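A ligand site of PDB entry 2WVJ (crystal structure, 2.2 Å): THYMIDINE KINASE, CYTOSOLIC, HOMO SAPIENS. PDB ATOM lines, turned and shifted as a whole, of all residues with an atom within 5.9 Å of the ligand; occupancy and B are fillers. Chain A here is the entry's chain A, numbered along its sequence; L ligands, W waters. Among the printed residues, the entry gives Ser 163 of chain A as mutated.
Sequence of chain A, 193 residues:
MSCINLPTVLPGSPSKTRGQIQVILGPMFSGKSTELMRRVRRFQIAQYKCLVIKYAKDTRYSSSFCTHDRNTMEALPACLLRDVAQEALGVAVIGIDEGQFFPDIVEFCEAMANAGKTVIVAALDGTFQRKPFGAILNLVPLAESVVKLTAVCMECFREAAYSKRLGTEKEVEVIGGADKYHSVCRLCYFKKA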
ATOM      1  N   GLY A  26     -13.039 -17.423  -6.934  1.00  0.00           N
ATOM      2  CA  GLY A  26     -11.689 -16.945  -7.200  1.00  0.00           C
ATOM      3  C   GLY A  26     -11.615 -15.451  -6.991  1.00  0.00           C
ATOM      4  O   GLY A  26     -12.646 -14.797  -6.796  1.00  0.00           O
ATOM      5  N   PRO A  27     -10.397 -14.893  -7.048  1.00  0.00           N
ATOM      6  CA  PRO A  27     -10.231 -13.444  -6.940  1.00  0.00           C
ATOM      7  C   PRO A  27     -10.592 -12.790  -8.272  1.00  0.00           C
ATOM      8  O   PRO A  27     -10.988 -13.489  -9.220  1.00  0.00           O
ATOM      9  CB  PRO A  27      -8.738 -13.285  -6.671  1.00  0.00           C
ATOM     10  CG  PRO A  27      -8.115 -14.452  -7.364  1.00  0.00           C
ATOM     11  CD  PRO A  27      -9.096 -15.583  -7.205  1.00  0.00           C
ATOM     12  N   MET A  28     -10.457 -11.470  -8.331  1.00  0.00           N
ATOM     13  CA  MET A  28     -10.560 -10.769  -9.601  1.00  0.00           C
ATOM     14  C   MET A  28      -9.447 -11.224 -10.557  1.00  0.00           C
ATOM     15  O   MET A  28      -8.367 -11.674 -10.117  1.00  0.00           O
ATOM     16  CB  MET A  28     -10.499  -9.257  -9.368  1.00  0.00           C
ATOM     17  CG  MET A  28     -11.713  -8.707  -8.612  1.00  0.00           C
ATOM     18  SD  MET A  28     -11.746  -6.911  -8.465  1.00  0.00           S
ATOM     19  CE  MET A  28     -11.929  -6.411 -10.170  1.00  0.00           C
ATOM     20  N   PHE A  29      -9.732 -11.155 -11.856  1.00  0.00           N
ATOM     21  CA  PHE A  29      -8.771 -11.402 -12.945  1.00  0.00           C
ATOM     22  C   PHE A  29      -8.354 -12.872 -13.099  1.00  0.00           C
ATOM     23  O   PHE A  29      -7.340 -13.178 -13.742  1.00  0.00           O
ATOM     24  CB  PHE A  29      -7.549 -10.475 -12.816  1.00  0.00           C
ATOM     25  CG  PHE A  29      -7.907  -9.042 -12.498  1.00  0.00           C
ATOM     26  CD1 PHE A  29      -7.475  -8.452 -11.315  1.00  0.00           C
ATOM     27  CD2 PHE A  29      -8.701  -8.295 -13.366  1.00  0.00           C
ATOM     28  CE1 PHE A  29      -7.796  -7.133 -11.005  1.00  0.00           C
ATOM     29  CE2 PHE A  29      -9.039  -6.969 -13.063  1.00  0.00           C
ATOM     30  CZ  PHE A  29      -8.587  -6.388 -11.882  1.00  0.00           C
ATOM     31  N   SER A  30      -9.153 -13.780 -12.510  1.00  0.00           N
ATOM     32  CA  SER A  30      -8.894 -15.220 -12.581  1.00  0.00           C
ATOM     33  C   SER A  30      -9.714 -15.902 -13.687  1.00  0.00           C
ATOM     34  O   SER A  30      -9.561 -17.092 -13.937  1.00  0.00           O
ATOM     35  CB  SER A  30      -9.155 -15.881 -11.220  1.00  0.00           C
ATOM     36  OG  SER A  30     -10.500 -15.743 -10.808  1.00  0.00           O
ATOM     37  N   GLY A  31     -10.574 -15.125 -14.357  1.00  0.00           N
ATOM     38  CA  GLY A  31     -11.365 -15.593 -15.496  1.00  0.00           C
ATOM     39  C   GLY A  31     -12.561 -16.468 -15.146  1.00  0.00           C
ATOM     40  O   GLY A  31     -12.890 -17.399 -15.888  1.00  0.00           O
ATOM     41  N   LYS A  32     -13.202 -16.158 -14.023  1.00  0.00           N
ATOM     42  CA  LYS A  32     -14.387 -16.877 -13.540  1.00  0.00           C
ATOM     43  C   LYS A  32     -15.556 -16.861 -14.542  1.00  0.00           C
ATOM     44  O   LYS A  32     -16.215 -17.890 -14.749  1.00  0.00           O
ATOM     45  CB  LYS A  32     -14.873 -16.302 -12.196  1.00  0.00           C
ATOM     46  CG  LYS A  32     -13.815 -16.286 -11.085  1.00  0.00           C
ATOM     47  CD  LYS A  32     -14.327 -15.649  -9.783  1.00  0.00           C
ATOM     48  CE  LYS A  32     -14.841 -14.216  -9.973  1.00  0.00           C
ATOM     49  NZ  LYS A  32     -13.786 -13.230 -10.379  1.00  0.00           N
ATOM     50  N   SER A  33     -15.810 -15.717 -15.158  1.00  0.00           N
ATOM     51  CA  SER A  33     -16.932 -15.619 -16.108  1.00  0.00           C
ATOM     52  C   SER A  33     -16.606 -16.279 -17.454  1.00  0.00           C
ATOM     53  O   SER A  33     -17.513 -16.681 -18.173  1.00  0.00           O
ATOM     54  CB  SER A  33     -17.387 -14.167 -16.283  1.00  0.00           C
ATOM     55  OG  SER A  33     -16.357 -13.374 -16.818  1.00  0.00           O
ATOM     56  N   THR A  34     -15.313 -16.409 -17.756  1.00  0.00           N
ATOM     57  CA  THR A  34     -14.846 -17.171 -18.920  1.00  0.00           C
ATOM     58  C   THR A  34     -15.048 -18.670 -18.698  1.00  0.00           C
ATOM     59  O   THR A  34     -15.460 -19.381 -19.616  1.00  0.00           O
ATOM     60  CB  THR A  34     -13.367 -16.871 -19.259  1.00  0.00           C
ATOM     61  OG1 THR A  34     -13.202 -15.466 -19.485  1.00  0.00           O
ATOM     62  CG2 THR A  34     -12.910 -17.644 -20.499  1.00  0.00           C
ATOM     63  N   ASP A  58     -22.747  -3.634 -12.663  1.00  0.00           N
ATOM     64  CA  ASP A  58     -21.395  -3.718 -13.211  1.00  0.00           C
ATOM     65  C   ASP A  58     -21.500  -3.522 -14.724  1.00  0.00           C
ATOM     66  O   ASP A  58     -21.919  -4.414 -15.459  1.00  0.00           O
ATOM     67  CB  ASP A  58     -20.706  -5.041 -12.860  1.00  0.00           C
ATOM     68  CG  ASP A  58     -19.198  -4.998 -13.097  1.00  0.00           C
ATOM     69  OD1 ASP A  58     -18.755  -4.311 -14.053  1.00  0.00           O
ATOM     70  OD2 ASP A  58     -18.447  -5.635 -12.328  1.00  0.00           O
ATOM     71  N   ARG A  60     -18.890  -1.834 -16.998  1.00  0.00           N
ATOM     72  CA  ARG A  60     -17.605  -2.126 -17.676  1.00  0.00           C
ATOM     73  C   ARG A  60     -17.720  -2.723 -19.088  1.00  0.00           C
ATOM     74  O   ARG A  60     -17.621  -3.941 -19.286  1.00  0.00           O
ATOM     75  CB  ARG A  60     -16.705  -2.970 -16.766  1.00  0.00           C
ATOM     76  CG  ARG A  60     -16.035  -2.170 -15.656  1.00  0.00           C
ATOM     77  CD  ARG A  60     -15.919  -2.951 -14.355  1.00  0.00           C
ATOM     78  NE  ARG A  60     -14.777  -3.867 -14.336  1.00  0.00           N
ATOM     79  CZ  ARG A  60     -14.852  -5.179 -14.100  1.00  0.00           C
ATOM     80  NH1 ARG A  60     -16.023  -5.757 -13.865  1.00  0.00           N
ATOM     81  NH2 ARG A  60     -13.742  -5.910 -14.107  1.00  0.00           N
ATOM     82  N   ASP A  97     -23.412 -14.701 -13.427  1.00  0.00           N
ATOM     83  CA  ASP A  97     -22.137 -14.003 -13.312  1.00  0.00           C
ATOM     84  C   ASP A  97     -22.187 -12.964 -12.199  1.00  0.00           C
ATOM     85  O   ASP A  97     -23.197 -12.276 -12.024  1.00  0.00           O
ATOM     86  CB  ASP A  97     -21.757 -13.357 -14.643  1.00  0.00           C
ATOM     87  CG  ASP A  97     -20.356 -12.773 -14.615  1.00  0.00           C
ATOM     88  OD1 ASP A  97     -19.441 -13.416 -14.038  1.00  0.00           O
ATOM     89  OD2 ASP A  97     -20.158 -11.675 -15.175  1.00  0.00           O
ATOM     90  N   GLU A  98     -21.072 -12.845 -11.476  1.00  0.00           N
ATOM     91  CA  GLU A  98     -20.937 -11.936 -10.322  1.00  0.00           C
ATOM     92  C   GLU A  98     -22.019 -12.184  -9.280  1.00  0.00           C
ATOM     93  O   GLU A  98     -22.702 -11.257  -8.825  1.00  0.00           O
ATOM     94  CB  GLU A  98     -20.936 -10.464 -10.762  1.00  0.00           C
ATOM     95  CG  GLU A  98     -19.691 -10.061 -11.537  1.00  0.00           C
ATOM     96  CD  GLU A  98     -19.712  -8.587 -11.920  1.00  0.00           C
ATOM     97  OE1 GLU A  98     -20.110  -7.756 -11.090  1.00  0.00           O
ATOM     98  OE2 GLU A  98     -19.323  -8.281 -13.063  1.00  0.00           O
ATOM     99  N   GLY A  99     -22.171 -13.454  -8.896  1.00  0.00           N
ATOM    100  CA  GLY A  99     -23.226 -13.886  -7.991  1.00  0.00           C
ATOM    101  C   GLY A  99     -23.202 -13.263  -6.612  1.00  0.00           C
ATOM    102  O   GLY A  99     -24.225 -13.243  -5.915  1.00  0.00           O
ATOM    103  N   GLN A 100     -22.038 -12.740  -6.220  1.00  0.00           N
ATOM    104  CA  GLN A 100     -21.834 -12.112  -4.914  1.00  0.00           C
ATOM    105  C   GLN A 100     -22.738 -10.890  -4.705  1.00  0.00           C
ATOM    106  O   GLN A 100     -23.071 -10.567  -3.561  1.00  0.00           O
ATOM    107  CB  GLN A 100     -20.361 -11.720  -4.708  1.00  0.00           C
ATOM    108  CG  GLN A 100     -19.846 -10.569  -5.583  1.00  0.00           C
ATOM    109  CD  GLN A 100     -19.258 -11.023  -6.920  1.00  0.00           C
ATOM    110  OE1 GLN A 100     -19.338 -12.187  -7.280  1.00  0.00           O
ATOM    111  NE2 GLN A 100     -18.668 -10.091  -7.654  1.00  0.00           N
ATOM    112  N   PHE A 101     -23.110 -10.227  -5.796  1.00  0.00           N
ATOM    113  CA  PHE A 101     -23.902  -8.997  -5.745  1.00  0.00           C
ATOM    114  C   PHE A 101     -25.406  -9.234  -5.598  1.00  0.00           C
ATOM    115  O   PHE A 101     -26.154  -8.283  -5.360  1.00  0.00           O
ATOM    116  CB  PHE A 101     -23.624  -8.128  -6.971  1.00  0.00           C
ATOM    117  CG  PHE A 101     -22.276  -7.468  -6.964  1.00  0.00           C
ATOM    118  CD1 PHE A 101     -21.335  -7.755  -7.955  1.00  0.00           C
ATOM    119  CD2 PHE A 101     -21.937  -6.568  -5.957  1.00  0.00           C
ATOM    120  CE1 PHE A 101     -20.093  -7.159  -7.947  1.00  0.00           C
ATOM    121  CE2 PHE A 101     -20.683  -5.966  -5.947  1.00  0.00           C
ATOM    122  CZ  PHE A 101     -19.763  -6.255  -6.944  1.00  0.00           C
ATOM    123  N   ALA A 122     -20.521 -18.001 -11.264  1.00  0.00           N
ATOM    124  CA  ALA A 122     -19.215 -17.359 -11.139  1.00  0.00           C
ATOM    125  C   ALA A 122     -19.321 -16.247 -10.100  1.00  0.00           C
ATOM    126  O   ALA A 122     -20.249 -15.413 -10.163  1.00  0.00           O
ATOM    127  CB  ALA A 122     -18.743 -16.795 -12.467  1.00  0.00           C
ATOM    128  N   ALA A 123     -18.412 -16.253  -9.129  1.00  0.00           N
ATOM    129  CA  ALA A 123     -18.438 -15.260  -8.064  1.00  0.00           C
ATOM    130  C   ALA A 123     -17.121 -15.114  -7.303  1.00  0.00           C
ATOM    131  O   ALA A 123     -16.392 -16.084  -7.105  1.00  0.00           O
ATOM    132  CB  ALA A 123     -19.570 -15.566  -7.070  1.00  0.00           C
ATOM    133  N   LEU A 124     -16.845 -13.879  -6.905  1.00  0.00           N
ATOM    134  CA  LEU A 124     -15.809 -13.557  -5.926  1.00  0.00           C
ATOM    135  C   LEU A 124     -16.143 -14.233  -4.597  1.00  0.00           C
ATOM    136  O   LEU A 124     -17.267 -14.107  -4.091  1.00  0.00           O
ATOM    137  CB  LEU A 124     -15.766 -12.050  -5.709  1.00  0.00           C
ATOM    138  CG  LEU A 124     -14.720 -11.096  -6.326  1.00  0.00           C
ATOM    139  CD1 LEU A 124     -13.871 -11.700  -7.432  1.00  0.00           C
ATOM    140  CD2 LEU A 124     -15.396  -9.806  -6.773  1.00  0.00           C
ATOM    141  N   GLY A 126     -14.294 -13.522  -1.858  1.00  0.00           N
ATOM    142  CA  GLY A 126     -13.902 -12.537  -0.873  1.00  0.00           C
ATOM    143  C   GLY A 126     -13.916 -11.106  -1.374  1.00  0.00           C
ATOM    144  O   GLY A 126     -13.676 -10.849  -2.565  1.00  0.00           O
ATOM    145  N   THR A 127     -14.186 -10.183  -0.457  1.00  0.00           N
ATOM    146  CA  THR A 127     -14.069  -8.747  -0.704  1.00  0.00           C
ATOM    147  C   THR A 127     -12.597  -8.324  -0.696  1.00  0.00           C
ATOM    148  O   THR A 127     -11.716  -9.146  -0.416  1.00  0.00           O
ATOM    149  CB  THR A 127     -14.807  -7.921   0.372  1.00  0.00           C
ATOM    150  OG1 THR A 127     -14.162  -8.101   1.636  1.00  0.00           O
ATOM    151  CG2 THR A 127     -16.270  -8.339   0.494  1.00  0.00           C
ATOM    152  N   PHE A 128     -12.361  -7.039  -0.961  1.00  0.00           N
ATOM    153  CA  PHE A 128     -11.031  -6.429  -0.843  1.00  0.00           C
ATOM    154  C   PHE A 128     -10.387  -6.634   0.543  1.00  0.00           C
ATOM    155  O   PHE A 128      -9.174  -6.438   0.716  1.00  0.00           O
ATOM    156  CB  PHE A 128     -11.082  -4.930  -1.209  1.00  0.00           C
ATOM    157  CG  PHE A 128     -11.679  -4.044  -0.143  1.00  0.00           C
ATOM    158  CD1 PHE A 128     -10.852  -3.234   0.641  1.00  0.00           C
ATOM    159  CD2 PHE A 128     -13.055  -4.004   0.076  1.00  0.00           C
ATOM    160  CE1 PHE A 128     -11.388  -2.389   1.628  1.00  0.00           C
ATOM    161  CE2 PHE A 128     -13.601  -3.176   1.074  1.00  0.00           C
ATOM    162  CZ  PHE A 128     -12.769  -2.369   1.839  1.00  0.00           C
ATOM    163  N   GLN A 129     -11.202  -7.053   1.521  1.00  0.00           N
ATOM    164  CA  GLN A 129     -10.737  -7.292   2.889  1.00  0.00           C
ATOM    165  C   GLN A 129     -10.608  -8.782   3.213  1.00  0.00           C
ATOM    166  O   GLN A 129     -10.397  -9.145   4.376  1.00  0.00           O
ATOM    167  CB  GLN A 129     -11.675  -6.614   3.888  1.00  0.00           C
ATOM    168  CG  GLN A 129     -11.595  -5.095   3.848  1.00  0.00           C
ATOM    169  CD  GLN A 129     -12.430  -4.435   4.916  1.00  0.00           C
ATOM    170  OE1 GLN A 129     -11.949  -3.538   5.616  1.00  0.00           O
ATOM    171  NE2 GLN A 129     -13.685  -4.863   5.052  1.00  0.00           N
ATOM    172  N   PHE A 133     -17.984 -12.436   0.603  1.00  0.00           N
ATOM    173  CA  PHE A 133     -18.635 -11.408  -0.201  1.00  0.00           C
ATOM    174  C   PHE A 133     -20.139 -11.668  -0.251  1.00  0.00           C
ATOM    175  O   PHE A 133     -20.613 -12.527  -0.988  1.00  0.00           O
ATOM    176  CB  PHE A 133     -18.059 -11.407  -1.630  1.00  0.00           C
ATOM    177  CG  PHE A 133     -18.154 -10.063  -2.332  1.00  0.00           C
ATOM    178  CD1 PHE A 133     -17.072  -9.577  -3.047  1.00  0.00           C
ATOM    179  CD2 PHE A 133     -19.329  -9.302  -2.277  1.00  0.00           C
ATOM    180  CE1 PHE A 133     -17.147  -8.336  -3.700  1.00  0.00           C
ATOM    181  CE2 PHE A 133     -19.412  -8.081  -2.929  1.00  0.00           C
ATOM    182  CZ  PHE A 133     -18.324  -7.596  -3.631  1.00  0.00           C
ATOM    183  N   SER A 163      -8.037 -10.171  -3.864  1.00  0.00           N
ATOM    184  CA  SER A 163      -8.233  -8.904  -4.560  1.00  0.00           C
ATOM    185  C   SER A 163      -7.871  -7.727  -3.654  1.00  0.00           C
ATOM    186  O   SER A 163      -8.408  -7.581  -2.551  1.00  0.00           O
ATOM    187  CB  SER A 163      -9.678  -8.770  -5.033  1.00  0.00           C
ATOM    188  OG  SER A 163     -10.112  -9.917  -5.754  1.00  0.00           O
ATOM    189  N   ARG A 165      -7.723  -3.668  -3.140  1.00  0.00           N
ATOM    190  CA  ARG A 165      -8.187  -2.345  -3.538  1.00  0.00           C
ATOM    191  C   ARG A 165      -7.008  -1.384  -3.526  1.00  0.00           C
ATOM    192  O   ARG A 165      -6.226  -1.360  -2.579  1.00  0.00           O
ATOM    193  CB  ARG A 165      -9.309  -1.855  -2.612  1.00  0.00           C
ATOM    194  CG  ARG A 165      -9.758  -0.421  -2.878  1.00  0.00           C
ATOM    195  CD  ARG A 165     -11.087  -0.111  -2.217  1.00  0.00           C
ATOM    196  NE  ARG A 165     -12.159  -0.933  -2.766  1.00  0.00           N
ATOM    197  CZ  ARG A 165     -13.345  -1.112  -2.177  1.00  0.00           C
ATOM    198  NH1 ARG A 165     -13.607  -0.535  -1.019  1.00  0.00           N
ATOM    199  NH2 ARG A 165     -14.254  -1.875  -2.762  1.00  0.00           N
ATOM    200  N   GLU A 171     -16.471   1.408   1.428  1.00  0.00           N
ATOM    201  CA  GLU A 171     -17.632   0.564   1.142  1.00  0.00           C
ATOM    202  C   GLU A 171     -17.241  -0.676   0.326  1.00  0.00           C
ATOM    203  O   GLU A 171     -16.226  -0.681  -0.366  1.00  0.00           O
ATOM    204  CB  GLU A 171     -18.728   1.373   0.434  1.00  0.00           C
ATOM    205  CG  GLU A 171     -18.420   1.813  -1.008  1.00  0.00           C
ATOM    206  CD  GLU A 171     -17.678   3.146  -1.112  1.00  0.00           C
ATOM    207  OE1 GLU A 171     -17.014   3.570  -0.132  1.00  0.00           O
ATOM    208  OE2 GLU A 171     -17.772   3.780  -2.184  1.00  0.00           O
ATOM    209  N   VAL A 172     -18.051  -1.728   0.449  1.00  0.00           N
ATOM    210  CA  VAL A 172     -17.775  -2.988  -0.239  1.00  0.00           C
ATOM    211  C   VAL A 172     -17.965  -2.863  -1.754  1.00  0.00           C
ATOM    212  O   VAL A 172     -17.064  -3.195  -2.513  1.00  0.00           O
ATOM    213  CB  VAL A 172     -18.605  -4.164   0.361  1.00  0.00           C
ATOM    214  CG1 VAL A 172     -18.493  -5.410  -0.509  1.00  0.00           C
ATOM    215  CG2 VAL A 172     -18.140  -4.465   1.784  1.00  0.00           C
ATOM    216  N   GLU A 173     -19.128  -2.357  -2.189  1.00  0.00           N
ATOM    217  CA  GLU A 173     -19.411  -2.243  -3.624  1.00  0.00           C
ATOM    218  C   GLU A 173     -18.743  -1.022  -4.263  1.00  0.00           C
ATOM    219  O   GLU A 173     -19.225   0.102  -4.147  1.00  0.00           O
ATOM    220  CB  GLU A 173     -20.920  -2.288  -3.910  1.00  0.00           C
ATOM    221  CG  GLU A 173     -21.257  -2.318  -5.409  1.00  0.00           C
ATOM    222  CD  GLU A 173     -22.687  -2.755  -5.710  1.00  0.00           C
ATOM    223  OE1 GLU A 173     -23.140  -2.539  -6.846  1.00  0.00           O
ATOM    224  OE2 GLU A 173     -23.350  -3.331  -4.813  1.00  0.00           O
ATOM    225  N   VAL A 174     -17.624  -1.278  -4.947  1.00  0.00           N
ATOM    226  CA  VAL A 174     -16.941  -0.281  -5.761  1.00  0.00           C
ATOM    227  C   VAL A 174     -16.580  -0.954  -7.093  1.00  0.00           C
ATOM    228  O   VAL A 174     -15.645  -1.756  -7.162  1.00  0.00           O
ATOM    229  CB  VAL A 174     -15.664   0.291  -5.055  1.00  0.00           C
ATOM    230  CG1 VAL A 174     -14.898   1.258  -5.964  1.00  0.00           C
ATOM    231  CG2 VAL A 174     -16.038   0.989  -3.753  1.00  0.00           C
ATOM    232  N   ILE A 175     -17.350  -0.630  -8.126  1.00  0.00           N
ATOM    233  CA  ILE A 175     -17.190  -1.250  -9.447  1.00  0.00           C
ATOM    234  C   ILE A 175     -15.909  -0.736 -10.115  1.00  0.00           C
ATOM    235  O   ILE A 175     -15.563   0.442  -9.983  1.00  0.00           O
ATOM    236  CB  ILE A 175     -18.450  -0.994 -10.355  1.00  0.00           C
ATOM    237  CG1 ILE A 175     -19.746  -1.468  -9.667  1.00  0.00           C
ATOM    238  CG2 ILE A 175     -18.297  -1.637 -11.737  1.00  0.00           C
ATOM    239  CD1 ILE A 175     -19.806  -2.962  -9.273  1.00  0.00           C
ATOM    240  N   GLY A 176     -15.209  -1.631 -10.816  1.00  0.00           N
ATOM    241  CA  GLY A 176     -13.989  -1.257 -11.529  1.00  0.00           C
ATOM    242  C   GLY A 176     -13.043  -2.424 -11.790  1.00  0.00           C
ATOM    243  O   GLY A 176     -13.206  -3.503 -11.212  1.00  0.00           O
ATOM    244  N   GLY A 177     -12.061  -2.198 -12.656  1.00  0.00           N
ATOM    245  CA  GLY A 177     -11.101  -3.226 -13.045  1.00  0.00           C
ATOM    246  C   GLY A 177      -9.725  -3.008 -12.451  1.00  0.00           C
ATOM    247  O   GLY A 177      -9.583  -2.709 -11.260  1.00  0.00           O
ATOM    248  N   TYR A 181      -8.238  -2.200  -8.726  1.00  0.00           N
ATOM    249  CA  TYR A 181      -7.880  -3.424  -7.987  1.00  0.00           C
ATOM    250  C   TYR A 181      -6.672  -4.146  -8.583  1.00  0.00           C
ATOM    251  O   TYR A 181      -6.447  -4.091  -9.793  1.00  0.00           O
ATOM    252  CB  TYR A 181      -9.058  -4.404  -7.963  1.00  0.00           C
ATOM    253  CG  TYR A 181     -10.333  -3.930  -7.275  1.00  0.00           C
ATOM    254  CD1 TYR A 181     -11.345  -3.299  -7.996  1.00  0.00           C
ATOM    255  CD2 TYR A 181     -10.543  -4.166  -5.907  1.00  0.00           C
ATOM    256  CE1 TYR A 181     -12.522  -2.882  -7.383  1.00  0.00           C
ATOM    257  CE2 TYR A 181     -11.725  -3.746  -5.275  1.00  0.00           C
ATOM    258  CZ  TYR A 181     -12.711  -3.106  -6.022  1.00  0.00           C
ATOM    259  OH  TYR A 181     -13.869  -2.687  -5.425  1.00  0.00           O
HETATM  260  P1  LIG L   1     -15.867 -10.294 -10.688  1.00  0.00           P
HETATM  261  O1  LIG L   1     -16.855 -11.323 -10.178  1.00  0.00           O
HETATM  262  O2  LIG L   1     -14.443 -10.671 -10.409  1.00  0.00           O
HETATM  263  O3  LIG L   1     -16.070  -9.950 -12.240  1.00  0.00           O
HETATM  264  P2  LIG L   1     -16.032 -11.053 -13.418  1.00  0.00           P
HETATM  265  O4  LIG L   1     -17.343 -11.784 -13.442  1.00  0.00           O
HETATM  266  O5  LIG L   1     -15.770 -10.346 -14.735  1.00  0.00           O
HETATM  267  O6  LIG L   1     -14.840 -12.074 -13.021  1.00  0.00           O
HETATM  268  P3  LIG L   1     -13.602 -12.485 -13.989  1.00  0.00           P
HETATM  269  O7  LIG L   1     -12.839 -11.259 -14.428  1.00  0.00           O
HETATM  270  O8  LIG L   1     -14.166 -13.195 -15.191  1.00  0.00           O
HETATM  271  O9  LIG L   1     -12.650 -13.371 -13.226  1.00  0.00           O
HETATM  272  O10 LIG L   1     -16.241  -8.905  -9.971  1.00  0.00           O
HETATM  273  C1  LIG L   1     -15.549  -7.718 -10.297  1.00  0.00           C
HETATM  274  C2  LIG L   1     -16.374  -6.554  -9.795  1.00  0.00           C
HETATM  275  O11 LIG L   1     -16.547  -6.651  -8.379  1.00  0.00           O
HETATM  276  C3  LIG L   1     -15.627  -5.257 -10.093  1.00  0.00           C
HETATM  277  O12 LIG L   1     -16.545  -4.342 -10.681  1.00  0.00           O
HETATM  278  C4  LIG L   1     -15.169  -4.755  -8.745  1.00  0.00           C
HETATM  279  C5  LIG L   1     -16.142  -5.413  -7.781  1.00  0.00           C
HETATM  280  N1  LIG L   1     -15.601  -5.587  -6.423  1.00  0.00           N
HETATM  281  C6  LIG L   1     -16.244  -4.888  -5.366  1.00  0.00           C
HETATM  282  O13 LIG L   1     -17.227  -4.152  -5.620  1.00  0.00           O
HETATM  283  N2  LIG L   1     -15.814  -4.999  -4.099  1.00  0.00           N
HETATM  284  C7  LIG L   1     -14.754  -5.775  -3.792  1.00  0.00           C
HETATM  285  O14 LIG L   1     -14.362  -5.853  -2.596  1.00  0.00           O
HETATM  286  C8  LIG L   1     -14.068  -6.515  -4.880  1.00  0.00           C
HETATM  287  C9  LIG L   1     -12.872  -7.393  -4.585  1.00  0.00           C
HETATM  288  C10 LIG L   1     -14.541  -6.378  -6.188  1.00  0.00           C
HETATM  289  O   HOH W   1     -13.117 -13.557 -17.488  1.00  0.00           O
HETATM  290  O   HOH W   2     -17.968 -13.284 -11.625  1.00  0.00           O
HETATM  291  O   HOH W   3     -12.550  -9.761 -12.403  1.00  0.00           O
HETATM  292  O   HOH W   4     -10.407 -11.925 -15.919  1.00  0.00           O
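The backbone carbonyl oxygen (O) of Val 172 is in hydrogen-bond range of a nitrogen (N2) of the ligand (2.7 Å). The backbone NH of Gly 31 is in hydrogen-bond range of an oxygen (O9) of the ligand. The backbone carbonyl oxygen (O) of Gly 176 lies close to an oxygen (O12) of the ligand (3.5 Å). The backbone NH of Lys 32 is in hydrogen-bond range of an oxygen (O9) of the ligand. An oxygen (O8) of the ligand lies within hydrogen-bond range of the side-chain hydroxyl of Ser 33. O13 of the ligand is in hydrogen-bond range of N of Val 174 (3.0 Å). The side-chain carboxylate (OD2) of Asp 58 is in hydrogen-bond range of an oxygen (O12) of the ligand (2.8 Å). O4 of the ligand lies close to OD1 of Asp 97 (2.7 Å). The backbone NH (N) of Gly 176 is in hydrogen-bond range of an oxygen (O12) of the ligand. NZ of Lys 32 lies within salt-bridge range of O2 of the ligand. N of Ser 33 is in hydrogen-bond range of O8 of the ligand (3.0 Å). An oxygen (O1) of the ligand sits at hydrogen-bond distance from the side-chain amide nitrogen (NE2) of Gln 100, at 3.3 Å. OH of Tyr 181 sits close to N2 of the ligand. The backbone NH (N) of Phe 128 lies within hydrogen-bond range of an oxygen (O14) of the ligand (2.8 Å).
The side-chain hydroxyl (OG) of Ser 30 lies within hydrogen-bond range of the backbone carbonyl oxygen (O) of Pro 27 (2.8 Å). The backbone carbonyl oxygen (O) of Glu 171 lies within hydrogen-bond range of the guanidinium group (NH1) of Arg 165 (2.7 Å). The side-chain amino group of Lys 32 is in hydrogen-bond range of the backbone carbonyl oxygen of Pro 27, at 3.0 Å. The backbone carbonyl oxygen (O) of Val 172 is in hydrogen-bond range of the guanidinium group (NH2) of Arg 165, at 3.1 Å. OH of Tyr 181 sits at hydrogen-bond distance from O of Val 174 (2.7 Å). The side-chain hydroxyl (OH) of Tyr 181 sits at hydrogen-bond distance from the guanidinium group (NH2) of Arg 165, at 2.8 Å. N of Leu 124 sits at hydrogen-bond distance from OE1 of Gln 100 (3.0 Å). The guanidinium group (NH1) of Arg 60 is in salt-bridge range of the side-chain carboxylate (OD2) of Asp 58 (2.9 Å).
SD of Met 28 touches C10 of the ligand, at 3.6 Å. N of Phe 29 touches O9 of the ligand (3.9 Å). N of Ser 30 touches O9 of the ligand, at 3.6 Å. Arg 60 touches the ligand (NH1 to O12, 3.5 Å). CG of Glu 98 touches O1 of the ligand, at 3.4 Å. Phe 101 touches the ligand (CZ to O11, 3.5 Å). CD1 of Leu 124 touches O2 of the ligand (3.2 Å). Thr 127 touches the ligand. Phe 133 touches the ligand (CE1 to C7, 3.5 Å). Ser 163 touches the ligand (CB to C9, 3.5 Å). NH2 of Arg 165 touches N2 of the ligand, at 3.7 Å. Glu 173 touches the ligand. CA of Ile 175 touches O12 of the ligand, at 3.4 Å. Hydrophobic or aromatic side chains within 4 Å of the ligand: Met 28, Phe 101, Leu 124, Phe 128, Phe 133, Ile 175 and Tyr 181. Within 4 Å of the ligand: Met 28, Phe 29, Ser 30, Gly 31, Lys 32, Ser 33, Asp 58, Arg 60, Asp 97, Glu 98, Gln 100, Phe 101, Leu 124, Thr 127, Phe 128, Phe 133, Ser 163, Arg 165, Val 172, Glu 173, Val 174, Ile 175, Gly 176 and Tyr 181.
Water W2 lies within hydrogen-bond range of O4 of the ligand (2.4 Å), OD1 of Asp 97 (2.8 Å), N of Glu 98 (3.1 Å) and O of Ala 122 (3.4 Å). Water W3 bridges O7 of the ligand (2.5 Å) and N of Phe 29 (3.2 Å). Water W1 lies within hydrogen-bond range of an oxygen (O8) of the ligand (2.6 Å), the side-chain hydroxyl of Thr 34 (2.8 Å) and the side-chain hydroxyl of Ser 33 (3.3 Å).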
